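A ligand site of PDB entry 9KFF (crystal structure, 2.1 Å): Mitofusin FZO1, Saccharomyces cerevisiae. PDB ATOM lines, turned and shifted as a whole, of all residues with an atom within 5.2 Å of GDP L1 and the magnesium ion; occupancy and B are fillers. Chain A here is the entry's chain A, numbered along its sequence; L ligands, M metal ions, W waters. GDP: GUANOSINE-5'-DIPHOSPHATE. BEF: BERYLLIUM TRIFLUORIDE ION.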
ATOM      1  N   ASP A 109     -23.272 -13.072  -7.542  1.00  0.00           N
ATOM      2  CA  ASP A 109     -23.425 -12.851  -6.100  1.00  0.00           C
ATOM      3  C   ASP A 109     -24.741 -12.143  -5.799  1.00  0.00           C
ATOM      4  O   ASP A 109     -25.336 -11.508  -6.666  1.00  0.00           O
ATOM      5  CB  ASP A 109     -22.256 -12.026  -5.553  1.00  0.00           C
ATOM      6  CG  ASP A 109     -21.039 -12.860  -5.214  1.00  0.00           C
ATOM      7  OD1 ASP A 109     -21.113 -14.097  -5.371  1.00  0.00           O
ATOM      8  OD2 ASP A 109     -19.988 -12.276  -4.799  1.00  0.00           O
ATOM      9  N   VAL A 110     -25.221 -12.283  -4.552  1.00  0.00           N
ATOM     10  CA  VAL A 110     -26.365 -11.495  -4.086  1.00  0.00           C
ATOM     11  C   VAL A 110     -26.078 -10.009  -4.297  1.00  0.00           C
ATOM     12  O   VAL A 110     -24.951  -9.548  -4.128  1.00  0.00           O
ATOM     13  CB  VAL A 110     -26.664 -11.780  -2.594  1.00  0.00           C
ATOM     14  CG1 VAL A 110     -25.425 -11.511  -1.716  1.00  0.00           C
ATOM     15  CG2 VAL A 110     -27.815 -10.883  -2.074  1.00  0.00           C
ATOM     16  N   ASN A 111     -27.106  -9.249  -4.696  1.00  0.00           N
ATOM     17  CA  ASN A 111     -27.021  -7.789  -4.788  1.00  0.00           C
ATOM     18  C   ASN A 111     -26.084  -7.304  -5.893  1.00  0.00           C
ATOM     19  O   ASN A 111     -25.561  -6.193  -5.817  1.00  0.00           O
ATOM     20  CB  ASN A 111     -26.580  -7.156  -3.459  1.00  0.00           C
ATOM     21  CG  ASN A 111     -27.709  -6.992  -2.509  1.00  0.00           C
ATOM     22  OD1 ASN A 111     -28.884  -6.962  -2.907  1.00  0.00           O
ATOM     23  ND2 ASN A 111     -27.372  -6.846  -1.230  1.00  0.00           N
ATOM     24  N   THR A 112     -25.825  -8.094  -6.923  1.00  0.00           N
ATOM     25  CA  THR A 112     -25.030  -7.570  -8.026  1.00  0.00           C
ATOM     26  C   THR A 112     -25.873  -6.851  -9.087  1.00  0.00           C
ATOM     27  O   THR A 112     -25.306  -6.202  -9.959  1.00  0.00           O
ATOM     28  CB  THR A 112     -24.242  -8.687  -8.701  1.00  0.00           C
ATOM     29  OG1 THR A 112     -25.099  -9.808  -8.973  1.00  0.00           O
ATOM     30  CG2 THR A 112     -23.113  -9.126  -7.794  1.00  0.00           C
ATOM     31  N   GLY A 113     -27.205  -6.984  -9.029  1.00  0.00           N
ATOM     32  CA  GLY A 113     -28.066  -6.378 -10.037  1.00  0.00           C
ATOM     33  C   GLY A 113     -28.650  -7.389 -11.016  1.00  0.00           C
ATOM     34  O   GLY A 113     -28.932  -7.040 -12.163  1.00  0.00           O
ATOM     35  N   LYS A 114     -28.816  -8.656 -10.599  1.00  0.00           N
ATOM     36  CA  LYS A 114     -29.319  -9.680 -11.507  1.00  0.00           C
ATOM     37  C   LYS A 114     -30.728  -9.350 -11.949  1.00  0.00           C
ATOM     38  O   LYS A 114     -31.027  -9.365 -13.154  1.00  0.00           O
ATOM     39  CB  LYS A 114     -29.315 -11.075 -10.854  1.00  0.00           C
ATOM     40  CG  LYS A 114     -27.912 -11.639 -10.453  1.00  0.00           C
ATOM     41  CD  LYS A 114     -28.040 -12.960  -9.680  1.00  0.00           C
ATOM     42  CE  LYS A 114     -28.785 -12.806  -8.379  1.00  0.00           C
ATOM     43  NZ  LYS A 114     -28.043 -11.961  -7.375  1.00  0.00           N
ATOM     44  N   SER A 115     -31.613  -9.022 -10.994  1.00  0.00           N
ATOM     45  CA  SER A 115     -33.004  -8.779 -11.327  1.00  0.00           C
ATOM     46  C   SER A 115     -33.148  -7.475 -12.114  1.00  0.00           C
ATOM     47  O   SER A 115     -33.988  -7.379 -13.012  1.00  0.00           O
ATOM     48  CB  SER A 115     -33.855  -8.748 -10.055  1.00  0.00           C
ATOM     49  OG  SER A 115     -33.752  -9.990  -9.362  1.00  0.00           O
ATOM     50  N   ALA A 116     -32.335  -6.481 -11.775  1.00  0.00           N
ATOM     51  CA  ALA A 116     -32.305  -5.236 -12.547  1.00  0.00           C
ATOM     52  C   ALA A 116     -31.887  -5.496 -13.991  1.00  0.00           C
ATOM     53  O   ALA A 116     -32.420  -4.895 -14.929  1.00  0.00           O
ATOM     54  CB  ALA A 116     -31.337  -4.231 -11.894  1.00  0.00           C
ATOM     55  N   PRO A 128     -38.771  -8.224  -8.833  1.00  0.00           N
ATOM     56  CA  PRO A 128     -38.447  -7.458  -7.625  1.00  0.00           C
ATOM     57  C   PRO A 128     -36.954  -7.167  -7.546  1.00  0.00           C
ATOM     58  O   PRO A 128     -36.110  -8.048  -7.729  1.00  0.00           O
ATOM     59  CB  PRO A 128     -38.926  -8.377  -6.492  1.00  0.00           C
ATOM     60  CG  PRO A 128     -40.126  -9.098  -7.144  1.00  0.00           C
ATOM     61  CD  PRO A 128     -39.643  -9.388  -8.539  1.00  0.00           C
ATOM     62  N   GLU A 129     -36.651  -5.894  -7.300  1.00  0.00           N
ATOM     63  CA  GLU A 129     -35.311  -5.330  -7.315  1.00  0.00           C
ATOM     64  C   GLU A 129     -35.208  -4.506  -6.040  1.00  0.00           C
ATOM     65  O   GLU A 129     -36.127  -3.752  -5.720  1.00  0.00           O
ATOM     66  CB  GLU A 129     -35.109  -4.506  -8.597  1.00  0.00           C
ATOM     67  CG  GLU A 129     -33.938  -3.550  -8.632  1.00  0.00           C
ATOM     68  CD  GLU A 129     -33.910  -2.674  -9.900  1.00  0.00           C
ATOM     69  OE1 GLU A 129     -34.677  -2.951 -10.863  1.00  0.00           O
ATOM     70  OE2 GLU A 129     -33.139  -1.698  -9.904  1.00  0.00           O
ATOM     71  N   ASP A 130     -34.127  -4.702  -5.267  1.00  0.00           N
ATOM     72  CA  ASP A 130     -34.102  -4.099  -3.945  1.00  0.00           C
ATOM     73  C   ASP A 130     -32.663  -4.032  -3.441  1.00  0.00           C
ATOM     74  O   ASP A 130     -31.814  -4.849  -3.801  1.00  0.00           O
ATOM     75  CB  ASP A 130     -34.971  -4.902  -2.947  1.00  0.00           C
ATOM     76  CG  ASP A 130     -35.144  -4.178  -1.598  1.00  0.00           C
ATOM     77  OD1 ASP A 130     -35.622  -3.018  -1.572  1.00  0.00           O
ATOM     78  OD2 ASP A 130     -34.710  -4.742  -0.570  1.00  0.00           O
ATOM     79  N   GLN A 131     -32.413  -3.035  -2.602  1.00  0.00           N
ATOM     80  CA  GLN A 131     -31.083  -2.861  -2.023  1.00  0.00           C
ATOM     81  C   GLN A 131     -30.644  -4.065  -1.172  1.00  0.00           C
ATOM     82  O   GLN A 131     -29.467  -4.437  -1.144  1.00  0.00           O
ATOM     83  CB  GLN A 131     -31.086  -1.577  -1.205  1.00  0.00           C
ATOM     84  CG  GLN A 131     -29.738  -1.151  -0.629  1.00  0.00           C
ATOM     85  CD  GLN A 131     -29.846   0.188   0.070  1.00  0.00           C
ATOM     86  OE1 GLN A 131     -30.896   0.530   0.602  1.00  0.00           O
ATOM     87  NE2 GLN A 131     -28.782   0.960   0.026  1.00  0.00           N
ATOM     88  N   CYS A 134     -33.008 -10.242  -1.941  1.00  0.00           N
ATOM     89  CA  CYS A 134     -34.375 -10.219  -2.442  1.00  0.00           C
ATOM     90  C   CYS A 134     -34.767 -11.549  -3.086  1.00  0.00           C
ATOM     91  O   CYS A 134     -35.673 -12.253  -2.597  1.00  0.00           O
ATOM     92  CB  CYS A 134     -34.506  -9.059  -3.427  1.00  0.00           C
ATOM     93  SG  CYS A 134     -36.116  -8.772  -4.090  1.00  0.00           S
ATOM     94  N   THR A 135     -34.119 -11.930  -4.184  1.00  0.00           N
ATOM     95  CA  THR A 135     -34.581 -13.075  -4.964  1.00  0.00           C
ATOM     96  C   THR A 135     -34.134 -14.381  -4.295  1.00  0.00           C
ATOM     97  O   THR A 135     -32.956 -14.717  -4.321  1.00  0.00           O
ATOM     98  CB  THR A 135     -34.061 -12.956  -6.391  1.00  0.00           C
ATOM     99  OG1 THR A 135     -34.182 -11.587  -6.835  1.00  0.00           O
ATOM    100  CG2 THR A 135     -34.853 -13.870  -7.342  1.00  0.00           C
ATOM    101  N   ASP A 227     -33.957 -15.725 -13.688  1.00  0.00           N
ATOM    102  CA  ASP A 227     -33.351 -14.832 -12.704  1.00  0.00           C
ATOM    103  C   ASP A 227     -32.932 -15.681 -11.512  1.00  0.00           C
ATOM    104  O   ASP A 227     -33.758 -16.420 -10.959  1.00  0.00           O
ATOM    105  CB  ASP A 227     -34.351 -13.736 -12.302  1.00  0.00           C
ATOM    106  CG  ASP A 227     -33.779 -12.706 -11.319  1.00  0.00           C
ATOM    107  OD1 ASP A 227     -32.543 -12.565 -11.183  1.00  0.00           O
ATOM    108  OD2 ASP A 227     -34.606 -11.979 -10.714  1.00  0.00           O
ATOM    109  N   SER A 228     -31.644 -15.659 -11.176  1.00  0.00           N
ATOM    110  CA  SER A 228     -31.187 -16.603 -10.180  1.00  0.00           C
ATOM    111  C   SER A 228     -31.261 -15.994  -8.772  1.00  0.00           C
ATOM    112  O   SER A 228     -31.101 -14.784  -8.585  1.00  0.00           O
ATOM    113  CB  SER A 228     -29.747 -17.021 -10.481  1.00  0.00           C
ATOM    114  OG  SER A 228     -29.249 -17.973  -9.546  1.00  0.00           O
ATOM    115  N   LYS A 284     -22.148  -4.468 -13.318  1.00  0.00           N
ATOM    116  CA  LYS A 284     -23.064  -3.456 -12.839  1.00  0.00           C
ATOM    117  C   LYS A 284     -22.410  -2.660 -11.713  1.00  0.00           C
ATOM    118  O   LYS A 284     -21.401  -3.071 -11.123  1.00  0.00           O
ATOM    119  CB  LYS A 284     -24.400  -4.095 -12.403  1.00  0.00           C
ATOM    120  CG  LYS A 284     -25.064  -4.878 -13.566  1.00  0.00           C
ATOM    121  CD  LYS A 284     -26.575  -5.161 -13.355  1.00  0.00           C
ATOM    122  CE  LYS A 284     -27.508  -4.205 -14.138  1.00  0.00           C
ATOM    123  NZ  LYS A 284     -27.342  -2.789 -13.708  1.00  0.00           N
ATOM    124  N   LYS A 285     -22.986  -1.486 -11.452  1.00  0.00           N
ATOM    125  CA  LYS A 285     -22.513  -0.531 -10.453  1.00  0.00           C
ATOM    126  C   LYS A 285     -21.180   0.082 -10.836  1.00  0.00           C
ATOM    127  O   LYS A 285     -20.454   0.596  -9.984  1.00  0.00           O
ATOM    128  CB  LYS A 285     -22.466  -1.167  -9.055  1.00  0.00           C
ATOM    129  CG  LYS A 285     -23.887  -1.524  -8.596  1.00  0.00           C
ATOM    130  CD  LYS A 285     -23.918  -2.305  -7.302  1.00  0.00           C
ATOM    131  CE  LYS A 285     -25.344  -2.767  -7.025  1.00  0.00           C
ATOM    132  NZ  LYS A 285     -25.493  -3.147  -5.593  1.00  0.00           N
ATOM    133  N   PHE A 286     -20.856   0.065 -12.125  1.00  0.00           N
ATOM    134  CA  PHE A 286     -19.654   0.742 -12.579  1.00  0.00           C
ATOM    135  C   PHE A 286     -19.811   2.241 -12.454  1.00  0.00           C
ATOM    136  O   PHE A 286     -18.814   2.953 -12.254  1.00  0.00           O
ATOM    137  CB  PHE A 286     -19.338   0.335 -14.008  1.00  0.00           C
ATOM    138  CG  PHE A 286     -17.931   0.628 -14.447  1.00  0.00           C
ATOM    139  CD1 PHE A 286     -16.854  -0.003 -13.844  1.00  0.00           C
ATOM    140  CD2 PHE A 286     -17.687   1.489 -15.502  1.00  0.00           C
ATOM    141  CE1 PHE A 286     -15.572   0.232 -14.264  1.00  0.00           C
ATOM    142  CE2 PHE A 286     -16.377   1.729 -15.934  1.00  0.00           C
ATOM    143  CZ  PHE A 286     -15.337   1.101 -15.313  1.00  0.00           C
ATOM    144  N   ASP A 287     -21.053   2.735 -12.547  1.00  0.00           N
ATOM    145  CA  ASP A 287     -21.332   4.157 -12.372  1.00  0.00           C
ATOM    146  C   ASP A 287     -20.861   4.666 -11.014  1.00  0.00           C
ATOM    147  O   ASP A 287     -20.610   5.864 -10.864  1.00  0.00           O
ATOM    148  CB  ASP A 287     -22.830   4.458 -12.517  1.00  0.00           C
ATOM    149  CG  ASP A 287     -23.701   3.534 -11.670  1.00  0.00           C
ATOM    150  OD1 ASP A 287     -24.541   4.022 -10.864  1.00  0.00           O
ATOM    151  OD2 ASP A 287     -23.536   2.299 -11.778  1.00  0.00           O
ATOM    152  N   LYS A 288     -20.725   3.778 -10.013  1.00  0.00           N
ATOM    153  CA  LYS A 288     -20.324   4.186  -8.671  1.00  0.00           C
ATOM    154  C   LYS A 288     -18.809   4.226  -8.474  1.00  0.00           C
ATOM    155  O   LYS A 288     -18.339   4.689  -7.433  1.00  0.00           O
ATOM    156  CB  LYS A 288     -20.927   3.223  -7.649  1.00  0.00           C
ATOM    157  CG  LYS A 288     -22.427   3.311  -7.474  1.00  0.00           C
ATOM    158  CD  LYS A 288     -22.984   1.947  -7.077  1.00  0.00           C
ATOM    159  CE  LYS A 288     -23.044   1.723  -5.556  1.00  0.00           C
ATOM    160  NZ  LYS A 288     -24.448   1.847  -5.009  1.00  0.00           N
ATOM    161  N   VAL A 321     -22.910  -2.147 -17.645  1.00  0.00           N
ATOM    162  CA  VAL A 321     -24.321  -1.762 -17.787  1.00  0.00           C
ATOM    163  C   VAL A 321     -24.837  -1.268 -16.443  1.00  0.00           C
ATOM    164  O   VAL A 321     -25.098  -2.068 -15.545  1.00  0.00           O
ATOM    165  CB  VAL A 321     -25.167  -2.920 -18.317  1.00  0.00           C
ATOM    166  CG1 VAL A 321     -26.649  -2.600 -18.236  1.00  0.00           C
ATOM    167  CG2 VAL A 321     -24.776  -3.189 -19.777  1.00  0.00           C
ATOM    168  N   SER A 322     -25.029   0.046 -16.322  1.00  0.00           N
ATOM    169  CA  SER A 322     -25.468   0.622 -15.060  1.00  0.00           C
ATOM    170  C   SER A 322     -26.991   0.780 -14.944  1.00  0.00           C
ATOM    171  O   SER A 322     -27.482   1.176 -13.880  1.00  0.00           O
ATOM    172  CB  SER A 322     -24.816   1.987 -14.839  1.00  0.00           C
ATOM    173  OG  SER A 322     -25.148   2.850 -15.906  1.00  0.00           O
ATOM    174  N   LYS A 323     -27.746   0.464 -16.002  1.00  0.00           N
ATOM    175  CA  LYS A 323     -29.197   0.665 -15.949  1.00  0.00           C
ATOM    176  C   LYS A 323     -29.796  -0.047 -14.738  1.00  0.00           C
ATOM    177  O   LYS A 323     -29.462  -1.196 -14.447  1.00  0.00           O
ATOM    178  CB  LYS A 323     -29.857   0.149 -17.231  1.00  0.00           C
ATOM    179  CG  LYS A 323     -31.305   0.573 -17.407  1.00  0.00           C
ATOM    180  CD  LYS A 323     -31.821   0.224 -18.805  1.00  0.00           C
ATOM    181  CE  LYS A 323     -31.501   1.328 -19.801  1.00  0.00           C
ATOM    182  NZ  LYS A 323     -31.877   0.911 -21.190  1.00  0.00           N
ATOM    183  N   ASN A 324     -30.666   0.661 -14.019  1.00  0.00           N
ATOM    184  CA  ASN A 324     -31.295   0.128 -12.813  1.00  0.00           C
ATOM    185  C   ASN A 324     -32.531   0.957 -12.527  1.00  0.00           C
ATOM    186  O   ASN A 324     -32.715   2.038 -13.095  1.00  0.00           O
ATOM    187  CB  ASN A 324     -30.348   0.146 -11.607  1.00  0.00           C
ATOM    188  CG  ASN A 324     -30.069   1.574 -11.130  1.00  0.00           C
ATOM    189  OD1 ASN A 324     -30.784   2.108 -10.271  1.00  0.00           O
ATOM    190  ND2 ASN A 324     -29.044   2.186 -11.680  1.00  0.00           N
ATOM    191  N   GLY A 325     -33.344   0.471 -11.600  1.00  0.00           N
ATOM    192  CA  GLY A 325     -34.594   1.115 -11.267  1.00  0.00           C
ATOM    193  C   GLY A 325     -34.708   1.683  -9.864  1.00  0.00           C
ATOM    194  O   GLY A 325     -35.828   1.748  -9.345  1.00  0.00           O
ATOM    195  N   ASP A 326     -33.610   2.107  -9.231  1.00  0.00           N
ATOM    196  CA  ASP A 326     -33.724   2.680  -7.872  1.00  0.00           C
ATOM    197  C   ASP A 326     -33.073   4.059  -7.709  1.00  0.00           C
ATOM    198  O   ASP A 326     -31.993   4.333  -8.251  1.00  0.00           O
ATOM    199  CB  ASP A 326     -33.128   1.724  -6.816  1.00  0.00           C
ATOM    200  CG  ASP A 326     -34.099   0.592  -6.402  1.00  0.00           C
ATOM    201  OD1 ASP A 326     -35.319   0.703  -6.719  1.00  0.00           O
ATOM    202  OD2 ASP A 326     -33.657  -0.372  -5.717  1.00  0.00           O
HETATM  203  PB  GDP L   1     -29.845  -8.822  -7.325  1.00  0.00           P
HETATM  204  O1B GDP L   1     -28.576  -9.235  -7.765  1.00  0.00           O
HETATM  205  O2B GDP L   1     -30.931  -9.278  -8.082  1.00  0.00           O
HETATM  206  O3B GDP L   1     -30.036  -9.115  -5.954  1.00  0.00           O
HETATM  207  O3A GDP L   1     -29.806  -7.254  -7.466  1.00  0.00           O
HETATM  208  PA  GDP L   1     -31.001  -6.263  -7.656  1.00  0.00           P
HETATM  209  O1A GDP L   1     -31.983  -6.461  -6.660  1.00  0.00           O
HETATM  210  O2A GDP L   1     -31.399  -6.305  -8.984  1.00  0.00           O
HETATM  211  O5' GDP L   1     -30.311  -4.900  -7.454  1.00  0.00           O
HETATM  212  C5' GDP L   1     -29.795  -4.559  -6.205  1.00  0.00           C
HETATM  213  C4' GDP L   1     -29.784  -3.043  -6.015  1.00  0.00           C
HETATM  214  O4' GDP L   1     -28.814  -2.410  -6.813  1.00  0.00           O
HETATM  215  C3' GDP L   1     -31.089  -2.433  -6.408  1.00  0.00           C
HETATM  216  O3' GDP L   1     -31.306  -1.381  -5.530  1.00  0.00           O
HETATM  217  C2' GDP L   1     -30.821  -1.916  -7.797  1.00  0.00           C
HETATM  218  O2' GDP L   1     -31.654  -0.865  -8.150  1.00  0.00           O
HETATM  219  C1' GDP L   1     -29.395  -1.506  -7.713  1.00  0.00           C
HETATM  220  N9  GDP L   1     -28.621  -1.583  -8.956  1.00  0.00           N
HETATM  221  C8  GDP L   1     -28.567  -2.569  -9.808  1.00  0.00           C
HETATM  222  N7  GDP L   1     -27.721  -2.320 -10.795  1.00  0.00           N
HETATM  223  C5  GDP L   1     -27.200  -1.162 -10.568  1.00  0.00           C
HETATM  224  C6  GDP L   1     -26.231  -0.307 -11.231  1.00  0.00           C
HETATM  225  O6  GDP L   1     -25.702  -0.658 -12.262  1.00  0.00           O
HETATM  226  N1  GDP L   1     -25.971   0.859 -10.650  1.00  0.00           N
HETATM  227  C2  GDP L   1     -26.529   1.255  -9.526  1.00  0.00           C
HETATM  228  N2  GDP L   1     -26.181   2.432  -9.040  1.00  0.00           N
HETATM  229  N3  GDP L   1     -27.422   0.510  -8.884  1.00  0.00           N
HETATM  230  C4  GDP L   1     -27.790  -0.679  -9.348  1.00  0.00           C
HETATM  231 BE   BEF L   2     -30.858 -11.248  -4.733  1.00  0.00          BE
HETATM  232  F1  BEF L   2     -29.207 -11.393  -5.093  1.00  0.00           F
HETATM  233  F2  BEF L   2     -31.800 -11.088  -6.114  1.00  0.00           F
HETATM  234  F3  BEF L   2     -31.053  -9.924  -3.703  1.00  0.00           F
HETATM  235 MG    MG M   1     -32.638 -10.480  -7.611  1.00  0.00          MG
HETATM  236  O   HOH W   1     -33.496  -8.871  -6.748  1.00  0.00           O
HETATM  237  O   HOH W   2     -29.619   0.356  -4.546  1.00  0.00           O
HETATM  238  O   HOH W   3     -31.940 -11.995  -8.764  1.00  0.00           O
HETATM  239  O   HOH W   4     -27.207   0.993  -6.215  1.00  0.00           O
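Water W3 lies within hydrogen-bond range of the side-chain carboxylate (OD1) of Asp 227 (2.6 Å) and the backbone carbonyl oxygen (O) of Ser 228 (2.9 Å). Water W1 lies within hydrogen-bond range of O1A of GDP L1 (2.8 Å), O of Pro 128 (2.9 Å) and SG of Cys 134 (3.7 Å). Water W4 bridges N3 of GDP L1 (2.7 Å) and NZ of Lys 288 (3.1 Å).
Residues that only touch the magnesium ion: Asp 227 (3.97 Å). Three residues have an atom within 4 Å of the magnesium ion: Ser 115, Thr 135 and Asp 227. The nearest printed residue that does not touch the magnesium ion is Pro 128 (4.2 Å).
The backbone carbonyl oxygen of Ser 322 sits close to an oxygen (O6) of GDP L1, 3.0 Å away. Gln 131 touches GDP L1 (N to O3', 3.5 Å). Lys 288 touches GDP L1 (CD to N2, 3.8 Å). O of Val 321 touches O6 of GDP L1, at 3.6 Å. ND2 of Asn 324 touches C2 of GDP L1, at 3.4 Å. Hydrophobic or aromatic side chains within 4 Å of GDP L1: Ala 116. Within 4 Å of GDP L1: Asn 111, Thr 112, Gly 113, Lys 114, Ser 115, Ala 116, Glu 129, Asp 130, Gln 131, Lys 284, Lys 285, Asp 287, Lys 288, Val 321, Ser 322, Asn 324 and Asp 326.
The magnesium ion is bound by a fluorine (F2) of BEF L2 (1.8 Å). The magnesium ion is bound by water W1 (2.0 Å). Water W3 binds the magnesium ion. The magnesium ion is bound by OG1 of Thr 135, at 2.1 Å. The magnesium ion is bound by the side-chain hydroxyl (OG) of Ser 115 (2.1 Å). O2B of GDP L1 is bound to the magnesium ion. The magnesium ion has six donor atoms within binding distance.
O of Ser 322 sits at hydrogen-bond distance from ND2 of Asn 324, at 2.9 Å. OG1 of Thr 112 lies within hydrogen-bond range of O of Asp 109 (2.9 Å). The backbone carbonyl oxygen (O) of Pro 128 sits close to the side-chain hydroxyl (OG) of Ser 115 (3.5 Å). The backbone carbonyl oxygen of Asn 111 lies within hydrogen-bond range of the side-chain amino group of Lys 285 (3.1 Å). O of Val 321 sits at hydrogen-bond distance from NZ of Lys 284 (3.0 Å). The side-chain hydroxyl (OG) of Ser 115 lies close to the side-chain carboxylate (OD2) of Asp 227 (2.6 Å). OE2 of Glu 129 sits at hydrogen-bond distance from N of Gly 325 (2.8 Å). NZ of Lys 284 lies within hydrogen-bond range of O of Lys 323, at 2.8 Å.
BE of BEF L2 is bound by O3B of GDP L1, 2.6 Å away.
N of Thr 112 sits at hydrogen-bond distance from O1B of GDP L1 (3.1 Å). An oxygen (O3') of GDP L1 sits at hydrogen-bond distance from the side-chain carboxylate (OD2) of Asp 326 (2.6 Å). The side-chain amino group (NZ) of Lys 284 sits at hydrogen-bond distance from a nitrogen (N7) of GDP L1. A nitrogen (N2) of GDP L1 lies within hydrogen-bond range of the side-chain carboxylate (OD1) of Asp 287 (2.9 Å). The side-chain amino group (NZ) of Lys 114 lies within salt-bridge range of an oxygen (O1B) of GDP L1. An oxygen (O2') of GDP L1 lies within hydrogen-bond range of the side-chain carboxylate (OE2) of Glu 129 (2.4 Å). N of Ser 115 lies within hydrogen-bond range of O2A of GDP L1, 3.4 Å away. The backbone NH of Asn 111 lies within hydrogen-bond range of a fluorine (F1) of BEF L2, at 3.0 Å. N of Asp 130 sits at hydrogen-bond distance from O1A of GDP L1 (3.1 Å). O1B of GDP L1 lies within hydrogen-bond range of N of Gly 113 (2.9 Å). The backbone NH of Ala 116 sits at hydrogen-bond distance from an oxygen (O2A) of GDP L1 (2.9 Å). The backbone NH (N) of Thr 135 sits close to a fluorine (F2) of BEF L2. N of Lys 285 is in hydrogen-bond range of O6 of GDP L1 (3.0 Å). NZ of Lys 114 lies within hydrogen-bond range of F1 of BEF L2. O1B of GDP L1 sits at hydrogen-bond distance from N of Lys 114. O1B of GDP L1 is in hydrogen-bond range of N of Asn 111. The backbone NH (N) of Cys 134 sits at hydrogen-bond distance from a fluorine (F3) of BEF L2.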
